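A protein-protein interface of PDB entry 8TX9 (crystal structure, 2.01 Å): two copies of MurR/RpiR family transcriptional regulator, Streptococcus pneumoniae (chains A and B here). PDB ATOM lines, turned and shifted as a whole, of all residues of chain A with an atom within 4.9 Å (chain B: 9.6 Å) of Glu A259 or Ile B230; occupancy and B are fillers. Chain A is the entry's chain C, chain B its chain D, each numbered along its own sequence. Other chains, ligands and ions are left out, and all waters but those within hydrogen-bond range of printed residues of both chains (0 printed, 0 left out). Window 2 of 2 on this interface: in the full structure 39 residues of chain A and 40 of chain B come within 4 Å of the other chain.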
ATOM      1  N   LEU A 149       3.399 -13.725 -20.102  1.00  0.00           N
ATOM      2  CA  LEU A 149       3.848 -13.874 -21.471  1.00  0.00           C
ATOM      3  C   LEU A 149       2.976 -14.829 -22.251  1.00  0.00           C
ATOM      4  O   LEU A 149       3.361 -15.236 -23.356  1.00  0.00           O
ATOM      5  CB  LEU A 149       5.290 -14.387 -21.520  1.00  0.00           C
ATOM      6  CG  LEU A 149       6.313 -13.526 -20.785  1.00  0.00           C
ATOM      7  CD1 LEU A 149       7.685 -14.143 -20.980  1.00  0.00           C
ATOM      8  CD2 LEU A 149       6.313 -12.084 -21.203  1.00  0.00           C
ATOM      9  N   TYR A 247      13.908 -17.540 -18.593  1.00  0.00           N
ATOM     10  CA  TYR A 247      12.947 -16.530 -18.971  1.00  0.00           C
ATOM     11  C   TYR A 247      13.459 -15.690 -20.159  1.00  0.00           C
ATOM     12  O   TYR A 247      12.742 -15.467 -21.128  1.00  0.00           O
ATOM     13  CB  TYR A 247      12.673 -15.654 -17.758  1.00  0.00           C
ATOM     14  CG  TYR A 247      11.751 -14.490 -17.988  1.00  0.00           C
ATOM     15  CD1 TYR A 247      10.398 -14.629 -17.863  1.00  0.00           C
ATOM     16  CD2 TYR A 247      12.266 -13.227 -18.289  1.00  0.00           C
ATOM     17  CE1 TYR A 247       9.529 -13.579 -18.060  1.00  0.00           C
ATOM     18  CE2 TYR A 247      11.420 -12.146 -18.510  1.00  0.00           C
ATOM     19  CZ  TYR A 247      10.032 -12.329 -18.430  1.00  0.00           C
ATOM     20  OH  TYR A 247       9.179 -11.289 -18.589  1.00  0.00           O
ATOM     21  N   LEU A 251      11.706 -15.417 -23.676  1.00  0.00           N
ATOM     22  CA  LEU A 251      11.087 -14.193 -24.149  1.00  0.00           C
ATOM     23  C   LEU A 251      11.484 -13.892 -25.603  1.00  0.00           C
ATOM     24  O   LEU A 251      10.693 -13.309 -26.350  1.00  0.00           O
ATOM     25  CB  LEU A 251      11.473 -13.055 -23.240  1.00  0.00           C
ATOM     26  CG  LEU A 251      10.932 -11.738 -23.738  1.00  0.00           C
ATOM     27  CD1 LEU A 251       9.388 -11.795 -23.778  1.00  0.00           C
ATOM     28  CD2 LEU A 251      11.456 -10.683 -22.833  1.00  0.00           C
ATOM     29  N   ARG A 255       8.774 -13.310 -29.792  1.00  0.00           N
ATOM     30  CA  ARG A 255       8.700 -12.295 -28.751  1.00  0.00           C
ATOM     31  C   ARG A 255       7.508 -11.383 -28.945  1.00  0.00           C
ATOM     32  O   ARG A 255       6.886 -10.941 -27.967  1.00  0.00           O
ATOM     33  CB  ARG A 255       9.961 -11.458 -28.697  1.00  0.00           C
ATOM     34  CG  ARG A 255       9.946 -10.459 -27.530  1.00  0.00           C
ATOM     35  CD  ARG A 255      11.252  -9.663 -27.316  1.00  0.00           C
ATOM     36  NE  ARG A 255      10.986  -8.502 -26.462  1.00  0.00           N
ATOM     37  CZ  ARG A 255      11.868  -7.917 -25.668  1.00  0.00           C
ATOM     38  NH1 ARG A 255      13.107  -8.394 -25.533  1.00  0.00           N
ATOM     39  NH2 ARG A 255      11.516  -6.813 -25.022  1.00  0.00           N
ATOM     40  N   GLU A 256       7.235 -10.999 -30.204  1.00  0.00           N
ATOM     41  CA  GLU A 256       6.209  -9.985 -30.425  1.00  0.00           C
ATOM     42  C   GLU A 256       4.886 -10.377 -29.797  1.00  0.00           C
ATOM     43  O   GLU A 256       4.258  -9.551 -29.113  1.00  0.00           O
ATOM     44  CB  GLU A 256       6.051  -9.701 -31.922  1.00  0.00           C
ATOM     45  CG  GLU A 256       7.294  -9.108 -32.565  1.00  0.00           C
ATOM     46  CD  GLU A 256       8.014 -10.054 -33.527  1.00  0.00           C
ATOM     47  OE1 GLU A 256       8.258 -11.223 -33.150  1.00  0.00           O
ATOM     48  OE2 GLU A 256       8.252  -9.638 -34.701  1.00  0.00           O
ATOM     49  N   SER A 257       4.476 -11.635 -29.948  1.00  0.00           N
ATOM     50  CA  SER A 257       3.197 -12.070 -29.365  1.00  0.00           C
ATOM     51  C   SER A 257       3.235 -12.033 -27.837  1.00  0.00           C
ATOM     52  O   SER A 257       2.228 -11.703 -27.198  1.00  0.00           O
ATOM     53  CB  SER A 257       2.838 -13.476 -29.847  1.00  0.00           C
ATOM     54  OG  SER A 257       3.841 -14.423 -29.506  1.00  0.00           O
ATOM     55  N   LYS A 258       4.397 -12.380 -27.230  1.00  0.00           N
ATOM     56  CA  LYS A 258       4.497 -12.399 -25.770  1.00  0.00           C
ATOM     57  C   LYS A 258       4.507 -11.005 -25.184  1.00  0.00           C
ATOM     58  O   LYS A 258       3.845 -10.765 -24.158  1.00  0.00           O
ATOM     59  CB  LYS A 258       5.774 -13.168 -25.330  1.00  0.00           C
ATOM     60  CG  LYS A 258       5.792 -14.594 -25.829  1.00  0.00           C
ATOM     61  CD  LYS A 258       6.993 -15.439 -25.475  1.00  0.00           C
ATOM     62  CE  LYS A 258       6.685 -16.814 -25.995  1.00  0.00           C
ATOM     63  NZ  LYS A 258       7.790 -17.752 -26.139  1.00  0.00           N
ATOM     64  N   GLU A 259       5.230 -10.050 -25.838  1.00  0.00           N
ATOM     65  CA  GLU A 259       5.273  -8.675 -25.339  1.00  0.00           C
ATOM     66  C   GLU A 259       3.880  -8.019 -25.380  1.00  0.00           C
ATOM     67  O   GLU A 259       3.559  -7.159 -24.545  1.00  0.00           O
ATOM     68  CB  GLU A 259       6.359  -7.889 -26.140  1.00  0.00           C
ATOM     69  CG  GLU A 259       6.736  -6.467 -25.578  1.00  0.00           C
ATOM     70  CD  GLU A 259       8.274  -6.079 -25.605  1.00  0.00           C
ATOM     71  OE1 GLU A 259       9.082  -6.726 -26.292  1.00  0.00           O
ATOM     72  OE2 GLU A 259       8.671  -5.093 -24.928  1.00  0.00           O
ATOM     73  N   LYS A 260       3.053  -8.372 -26.364  1.00  0.00           N
ATOM     74  CA  LYS A 260       1.665  -7.868 -26.422  1.00  0.00           C
ATOM     75  C   LYS A 260       0.813  -8.401 -25.256  1.00  0.00           C
ATOM     76  O   LYS A 260       0.079  -7.661 -24.607  1.00  0.00           O
ATOM     77  CB  LYS A 260       1.032  -8.261 -27.787  1.00  0.00           C
ATOM     78  CG  LYS A 260      -0.542  -8.176 -27.907  1.00  0.00           C
ATOM     79  CD  LYS A 260      -1.135  -9.394 -28.752  1.00  0.00           C
ATOM     80  CE  LYS A 260      -0.455 -10.767 -28.258  1.00  0.00           C
ATOM     81  NZ  LYS A 260      -0.700 -12.076 -28.950  1.00  0.00           N
ATOM     82  N   ILE A 261       0.911  -9.691 -24.943  1.00  0.00           N
ATOM     83  CA  ILE A 261       0.153 -10.200 -23.789  1.00  0.00           C
ATOM     84  C   ILE A 261       0.621  -9.498 -22.526  1.00  0.00           C
ATOM     85  O   ILE A 261      -0.172  -8.969 -21.734  1.00  0.00           O
ATOM     86  CB  ILE A 261       0.309 -11.729 -23.691  1.00  0.00           C
ATOM     87  CG1 ILE A 261      -0.448 -12.400 -24.847  1.00  0.00           C
ATOM     88  CG2 ILE A 261      -0.221 -12.252 -22.369  1.00  0.00           C
ATOM     89  CD1 ILE A 261       0.185 -13.685 -25.363  1.00  0.00           C
ATOM     90  N   PHE A 262       1.924  -9.335 -22.403  1.00  0.00           N
ATOM     91  CA  PHE A 262       2.466  -8.723 -21.202  1.00  0.00           C
ATOM     92  C   PHE A 262       2.022  -7.294 -21.077  1.00  0.00           C
ATOM     93  O   PHE A 262       1.689  -6.828 -19.980  1.00  0.00           O
ATOM     94  CB  PHE A 262       3.981  -8.805 -21.279  1.00  0.00           C
ATOM     95  CG  PHE A 262       4.668  -8.245 -20.074  1.00  0.00           C
ATOM     96  CD1 PHE A 262       4.968  -9.059 -18.993  1.00  0.00           C
ATOM     97  CD2 PHE A 262       5.037  -6.921 -20.022  1.00  0.00           C
ATOM     98  CE1 PHE A 262       5.689  -8.557 -17.965  1.00  0.00           C
ATOM     99  CE2 PHE A 262       5.646  -6.391 -18.960  1.00  0.00           C
ATOM    100  CZ  PHE A 262       6.025  -7.199 -17.933  1.00  0.00           C
ATOM    101  N   ASN A 263       2.056  -6.562 -22.197  1.00  0.00           N
ATOM    102  CA  ASN A 263       1.617  -5.173 -22.213  1.00  0.00           C
ATOM    103  C   ASN A 263       0.112  -5.005 -21.987  1.00  0.00           C
ATOM    104  O   ASN A 263      -0.324  -3.926 -21.556  1.00  0.00           O
ATOM    105  CB  ASN A 263       2.058  -4.538 -23.542  1.00  0.00           C
ATOM    106  CG  ASN A 263       3.566  -4.199 -23.571  1.00  0.00           C
ATOM    107  OD1 ASN A 263       4.245  -4.164 -22.526  1.00  0.00           O
ATOM    108  ND2 ASN A 263       4.108  -4.014 -24.766  1.00  0.00           N
ATOM    109  N   ARG B  93      23.552 -10.660 -20.169  1.00  0.00           N
ATOM    110  CA  ARG B  93      22.650  -9.613 -19.658  1.00  0.00           C
ATOM    111  C   ARG B  93      22.047 -10.014 -18.329  1.00  0.00           C
ATOM    112  O   ARG B  93      22.054  -9.244 -17.368  1.00  0.00           O
ATOM    113  CB  ARG B  93      21.520  -9.326 -20.691  1.00  0.00           C
ATOM    114  CG  ARG B  93      20.539  -8.257 -20.244  1.00  0.00           C
ATOM    115  CD  ARG B  93      19.344  -8.165 -21.169  1.00  0.00           C
ATOM    116  NE  ARG B  93      18.265  -9.050 -20.748  1.00  0.00           N
ATOM    117  CZ  ARG B  93      17.416  -9.646 -21.575  1.00  0.00           C
ATOM    118  NH1 ARG B  93      17.538  -9.537 -22.886  1.00  0.00           N
ATOM    119  NH2 ARG B  93      16.420 -10.385 -21.075  1.00  0.00           N
ATOM    120  N   VAL B  94      21.557 -11.244 -18.251  1.00  0.00           N
ATOM    121  CA  VAL B  94      20.948 -11.708 -16.972  1.00  0.00           C
ATOM    122  C   VAL B  94      21.981 -11.687 -15.865  1.00  0.00           C
ATOM    123  O   VAL B  94      21.742 -11.203 -14.760  1.00  0.00           O
ATOM    124  CB  VAL B  94      20.351 -13.108 -17.169  1.00  0.00           C
ATOM    125  CG1 VAL B  94      19.982 -13.690 -15.803  1.00  0.00           C
ATOM    126  CG2 VAL B  94      19.129 -13.083 -18.142  1.00  0.00           C
ATOM    127  N   HIS B 224      16.297  -2.232 -10.221  1.00  0.00           N
ATOM    128  CA  HIS B 224      16.729  -3.117 -11.277  1.00  0.00           C
ATOM    129  C   HIS B 224      17.556  -2.303 -12.271  1.00  0.00           C
ATOM    130  O   HIS B 224      17.675  -1.076 -12.146  1.00  0.00           O
ATOM    131  CB  HIS B 224      15.521  -3.738 -11.948  1.00  0.00           C
ATOM    132  CG  HIS B 224      14.821  -4.728 -11.091  1.00  0.00           C
ATOM    133  ND1 HIS B 224      14.865  -6.089 -11.327  1.00  0.00           N
ATOM    134  CD2 HIS B 224      14.075  -4.561  -9.979  1.00  0.00           C
ATOM    135  CE1 HIS B 224      14.144  -6.713 -10.409  1.00  0.00           C
ATOM    136  NE2 HIS B 224      13.695  -5.812  -9.556  1.00  0.00           N
ATOM    137  N   GLN B 226      17.429  -3.089 -15.923  1.00  0.00           N
ATOM    138  CA  GLN B 226      16.947  -3.131 -17.275  1.00  0.00           C
ATOM    139  C   GLN B 226      15.916  -2.032 -17.473  1.00  0.00           C
ATOM    140  O   GLN B 226      15.005  -1.906 -16.646  1.00  0.00           O
ATOM    141  CB  GLN B 226      16.315  -4.473 -17.579  1.00  0.00           C
ATOM    142  CG  GLN B 226      17.322  -5.481 -17.940  1.00  0.00           C
ATOM    143  CD  GLN B 226      18.005  -5.132 -19.254  1.00  0.00           C
ATOM    144  OE1 GLN B 226      17.348  -4.878 -20.270  1.00  0.00           O
ATOM    145  NE2 GLN B 226      19.346  -5.127 -19.224  1.00  0.00           N
ATOM    146  N   PRO B 227      16.035  -1.253 -18.539  1.00  0.00           N
ATOM    147  CA  PRO B 227      15.030  -0.206 -18.773  1.00  0.00           C
ATOM    148  C   PRO B 227      13.627  -0.764 -18.938  1.00  0.00           C
ATOM    149  O   PRO B 227      12.702  -0.269 -18.301  1.00  0.00           O
ATOM    150  CB  PRO B 227      15.550   0.477 -20.036  1.00  0.00           C
ATOM    151  CG  PRO B 227      17.057   0.381 -19.922  1.00  0.00           C
ATOM    152  CD  PRO B 227      17.259  -1.039 -19.340  1.00  0.00           C
ATOM    153  N   SER B 228      13.452  -1.803 -19.746  1.00  0.00           N
ATOM    154  CA  SER B 228      12.116  -2.330 -20.014  1.00  0.00           C
ATOM    155  C   SER B 228      11.736  -3.316 -18.907  1.00  0.00           C
ATOM    156  O   SER B 228      12.557  -4.151 -18.470  1.00  0.00           O
ATOM    157  CB  SER B 228      12.039  -2.989 -21.404  1.00  0.00           C
ATOM    158  OG  SER B 228      12.865  -4.141 -21.580  1.00  0.00           O
ATOM    159  N   TYR B 229      10.521  -3.139 -18.390  1.00  0.00           N
ATOM    160  CA  TYR B 229      10.051  -3.934 -17.257  1.00  0.00           C
ATOM    161  C   TYR B 229      10.058  -5.405 -17.590  1.00  0.00           C
ATOM    162  O   TYR B 229      10.468  -6.263 -16.774  1.00  0.00           O
ATOM    163  CB  TYR B 229       8.668  -3.435 -16.819  1.00  0.00           C
ATOM    164  CG  TYR B 229       8.189  -4.029 -15.512  1.00  0.00           C
ATOM    165  CD1 TYR B 229       7.521  -5.236 -15.479  1.00  0.00           C
ATOM    166  CD2 TYR B 229       8.521  -3.427 -14.294  1.00  0.00           C
ATOM    167  CE1 TYR B 229       7.131  -5.826 -14.263  1.00  0.00           C
ATOM    168  CE2 TYR B 229       8.097  -3.968 -13.077  1.00  0.00           C
ATOM    169  CZ  TYR B 229       7.395  -5.174 -13.065  1.00  0.00           C
ATOM    170  OH  TYR B 229       6.980  -5.752 -11.870  1.00  0.00           O
ATOM    171  N   ILE B 230       9.669  -5.738 -18.815  1.00  0.00           N
ATOM    172  CA  ILE B 230       9.568  -7.168 -19.194  1.00  0.00           C
ATOM    173  C   ILE B 230      10.886  -7.913 -19.154  1.00  0.00           C
ATOM    174  O   ILE B 230      10.875  -9.159 -19.053  1.00  0.00           O
ATOM    175  CB  ILE B 230       8.929  -7.203 -20.603  1.00  0.00           C
ATOM    176  CG1 ILE B 230       8.438  -8.586 -20.968  1.00  0.00           C
ATOM    177  CG2 ILE B 230       9.899  -6.709 -21.682  1.00  0.00           C
ATOM    178  CD1 ILE B 230       7.583  -8.610 -22.292  1.00  0.00           C
ATOM    179  N   GLN B 231      12.039  -7.204 -19.317  1.00  0.00           N
ATOM    180  CA  GLN B 231      13.380  -7.828 -19.292  1.00  0.00           C
ATOM    181  C   GLN B 231      14.036  -7.837 -17.901  1.00  0.00           C
ATOM    182  O   GLN B 231      15.171  -8.284 -17.780  1.00  0.00           O
ATOM    183  CB  GLN B 231      14.361  -7.099 -20.323  1.00  0.00           C
ATOM    184  CG  GLN B 231      13.966  -7.356 -21.814  1.00  0.00           C
ATOM    185  CD  GLN B 231      14.926  -6.771 -22.885  1.00  0.00           C
ATOM    186  OE1 GLN B 231      14.694  -7.003 -24.067  1.00  0.00           O
ATOM    187  NE2 GLN B 231      15.997  -6.096 -22.456  1.00  0.00           N
ATOM    188  N   ARG B 232      13.357  -7.368 -16.870  1.00  0.00           N
ATOM    189  CA  ARG B 232      13.965  -7.264 -15.526  1.00  0.00           C
ATOM    190  C   ARG B 232      14.114  -8.642 -14.867  1.00  0.00           C
ATOM    191  O   ARG B 232      13.316  -9.522 -15.211  1.00  0.00           O
ATOM    192  CB  ARG B 232      13.134  -6.335 -14.650  1.00  0.00           C
ATOM    193  CG  ARG B 232      13.196  -4.882 -15.072  1.00  0.00           C
ATOM    194  CD  ARG B 232      12.504  -4.022 -14.045  1.00  0.00           C
ATOM    195  NE  ARG B 232      12.864  -2.628 -14.232  1.00  0.00           N
ATOM    196  CZ  ARG B 232      11.987  -1.677 -14.484  1.00  0.00           C
ATOM    197  NH1 ARG B 232      11.222  -1.216 -13.516  1.00  0.00           N
ATOM    198  NH2 ARG B 232      11.863  -1.211 -15.713  1.00  0.00           N
ATOM    199  N   ILE B 233      15.077  -8.814 -13.943  1.00  0.00           N
ATOM    200  CA  ILE B 233      15.322 -10.059 -13.153  1.00  0.00           C
ATOM    201  C   ILE B 233      14.104 -10.199 -12.254  1.00  0.00           C
ATOM    202  O   ILE B 233      13.349  -9.235 -12.160  1.00  0.00           O
ATOM    203  CB  ILE B 233      16.546  -9.921 -12.195  1.00  0.00           C
ATOM    204  CG1 ILE B 233      17.822  -9.399 -12.731  1.00  0.00           C
ATOM    205  CG2 ILE B 233      16.959 -11.220 -11.529  1.00  0.00           C
ATOM    206  CD1 ILE B 233      18.612  -8.704 -11.608  1.00  0.00           C
ATOM    207  N   SER B 234      13.955 -11.328 -11.551  1.00  0.00           N
ATOM    208  CA  SER B 234      12.908 -11.506 -10.528  1.00  0.00           C
ATOM    209  C   SER B 234      12.787 -10.270  -9.662  1.00  0.00           C
ATOM    210  O   SER B 234      13.799  -9.783  -9.157  1.00  0.00           O
ATOM    211  CB  SER B 234      13.247 -12.718  -9.682  1.00  0.00           C
ATOM    212  OG  SER B 234      12.680 -12.625  -8.399  1.00  0.00           O
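Among the printed residues, pairs that only touch across the chains: Leu A149 with Ile B230 (3.9 Å), Leu A251 with Ile B230 (3.95 Å), Arg A255 with Ile B230 (3.7 Å), Glu A259 with Ile B230 (3.8 Å), Phe A262 with Tyr B229 (3.5 Å) and Phe A262 with Ile B230 (3.7 Å).
The side-chain hydroxyl (OH) of Tyr A247 sits at hydrogen-bond distance from the backbone carbonyl oxygen (O) of Ile B230, at 2.8 Å. The guanidinium group of Arg A255 sits at hydrogen-bond distance from the side-chain amide oxygen of Gln B231 (2.6 Å).
Of the 12 printed residues of chain A, 6 touch a printed residue of chain B. Hydrophobic or aromatic side chains of chain A within 4 Å of the printed part of chain B: Leu A149, Tyr A247, Leu A251 and Phe A262. Of the 12 printed residues of chain B, 3 touch a printed residue of chain A. Among the printed residues, no Asp or Glu carboxylate lies within 4 Å of a Lys or Arg side-chain nitrogen of the other chain.
Of the printed residues of chain B, Tyr A247 touches Ile B230. Of the printed residues of chain B, Arg A255 touches Ile B230 and Gln B231. Ser A257 touches none of the printed residues of chain B. Lys A258 touches none of the printed residues of chain B. Of chain B, only Ile B230 (3.8 Å) comes within 4 Å of Glu A259. Of chain B, only Tyr B229 and Ile B230 come within 4 Å of Phe A262. Of chain A, only Leu A149, Tyr A247, Leu A251, Arg A255, Glu A259 and Phe A262 come within 4 Å of Ile B230. Printed residues of chain A within 4 Å of Gln B231: Arg A255 (2.6 Å). The nearest residue of chain B that does not touch Glu A259 is Ser B228 (5.3 Å). The nearest printed residue of chain B that does not touch Arg A255 is Ser B228 (4.6 Å).
The side-chain carboxylate of Glu A259 lies within salt-bridge range of the guanidinium group of Arg A255 (2.6 Å). The side-chain amide nitrogen of Gln B231 lies within hydrogen-bond range of the side-chain amide oxygen of Gln B226, at 2.8 Å. O of Glu A259 lies close to ND2 of Asn A263 (3.2 Å).
No position is printed for both chains. Of the 8 pairs that touch across the chains among the printed residues, none has its exchanged pair printed and touching as well.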
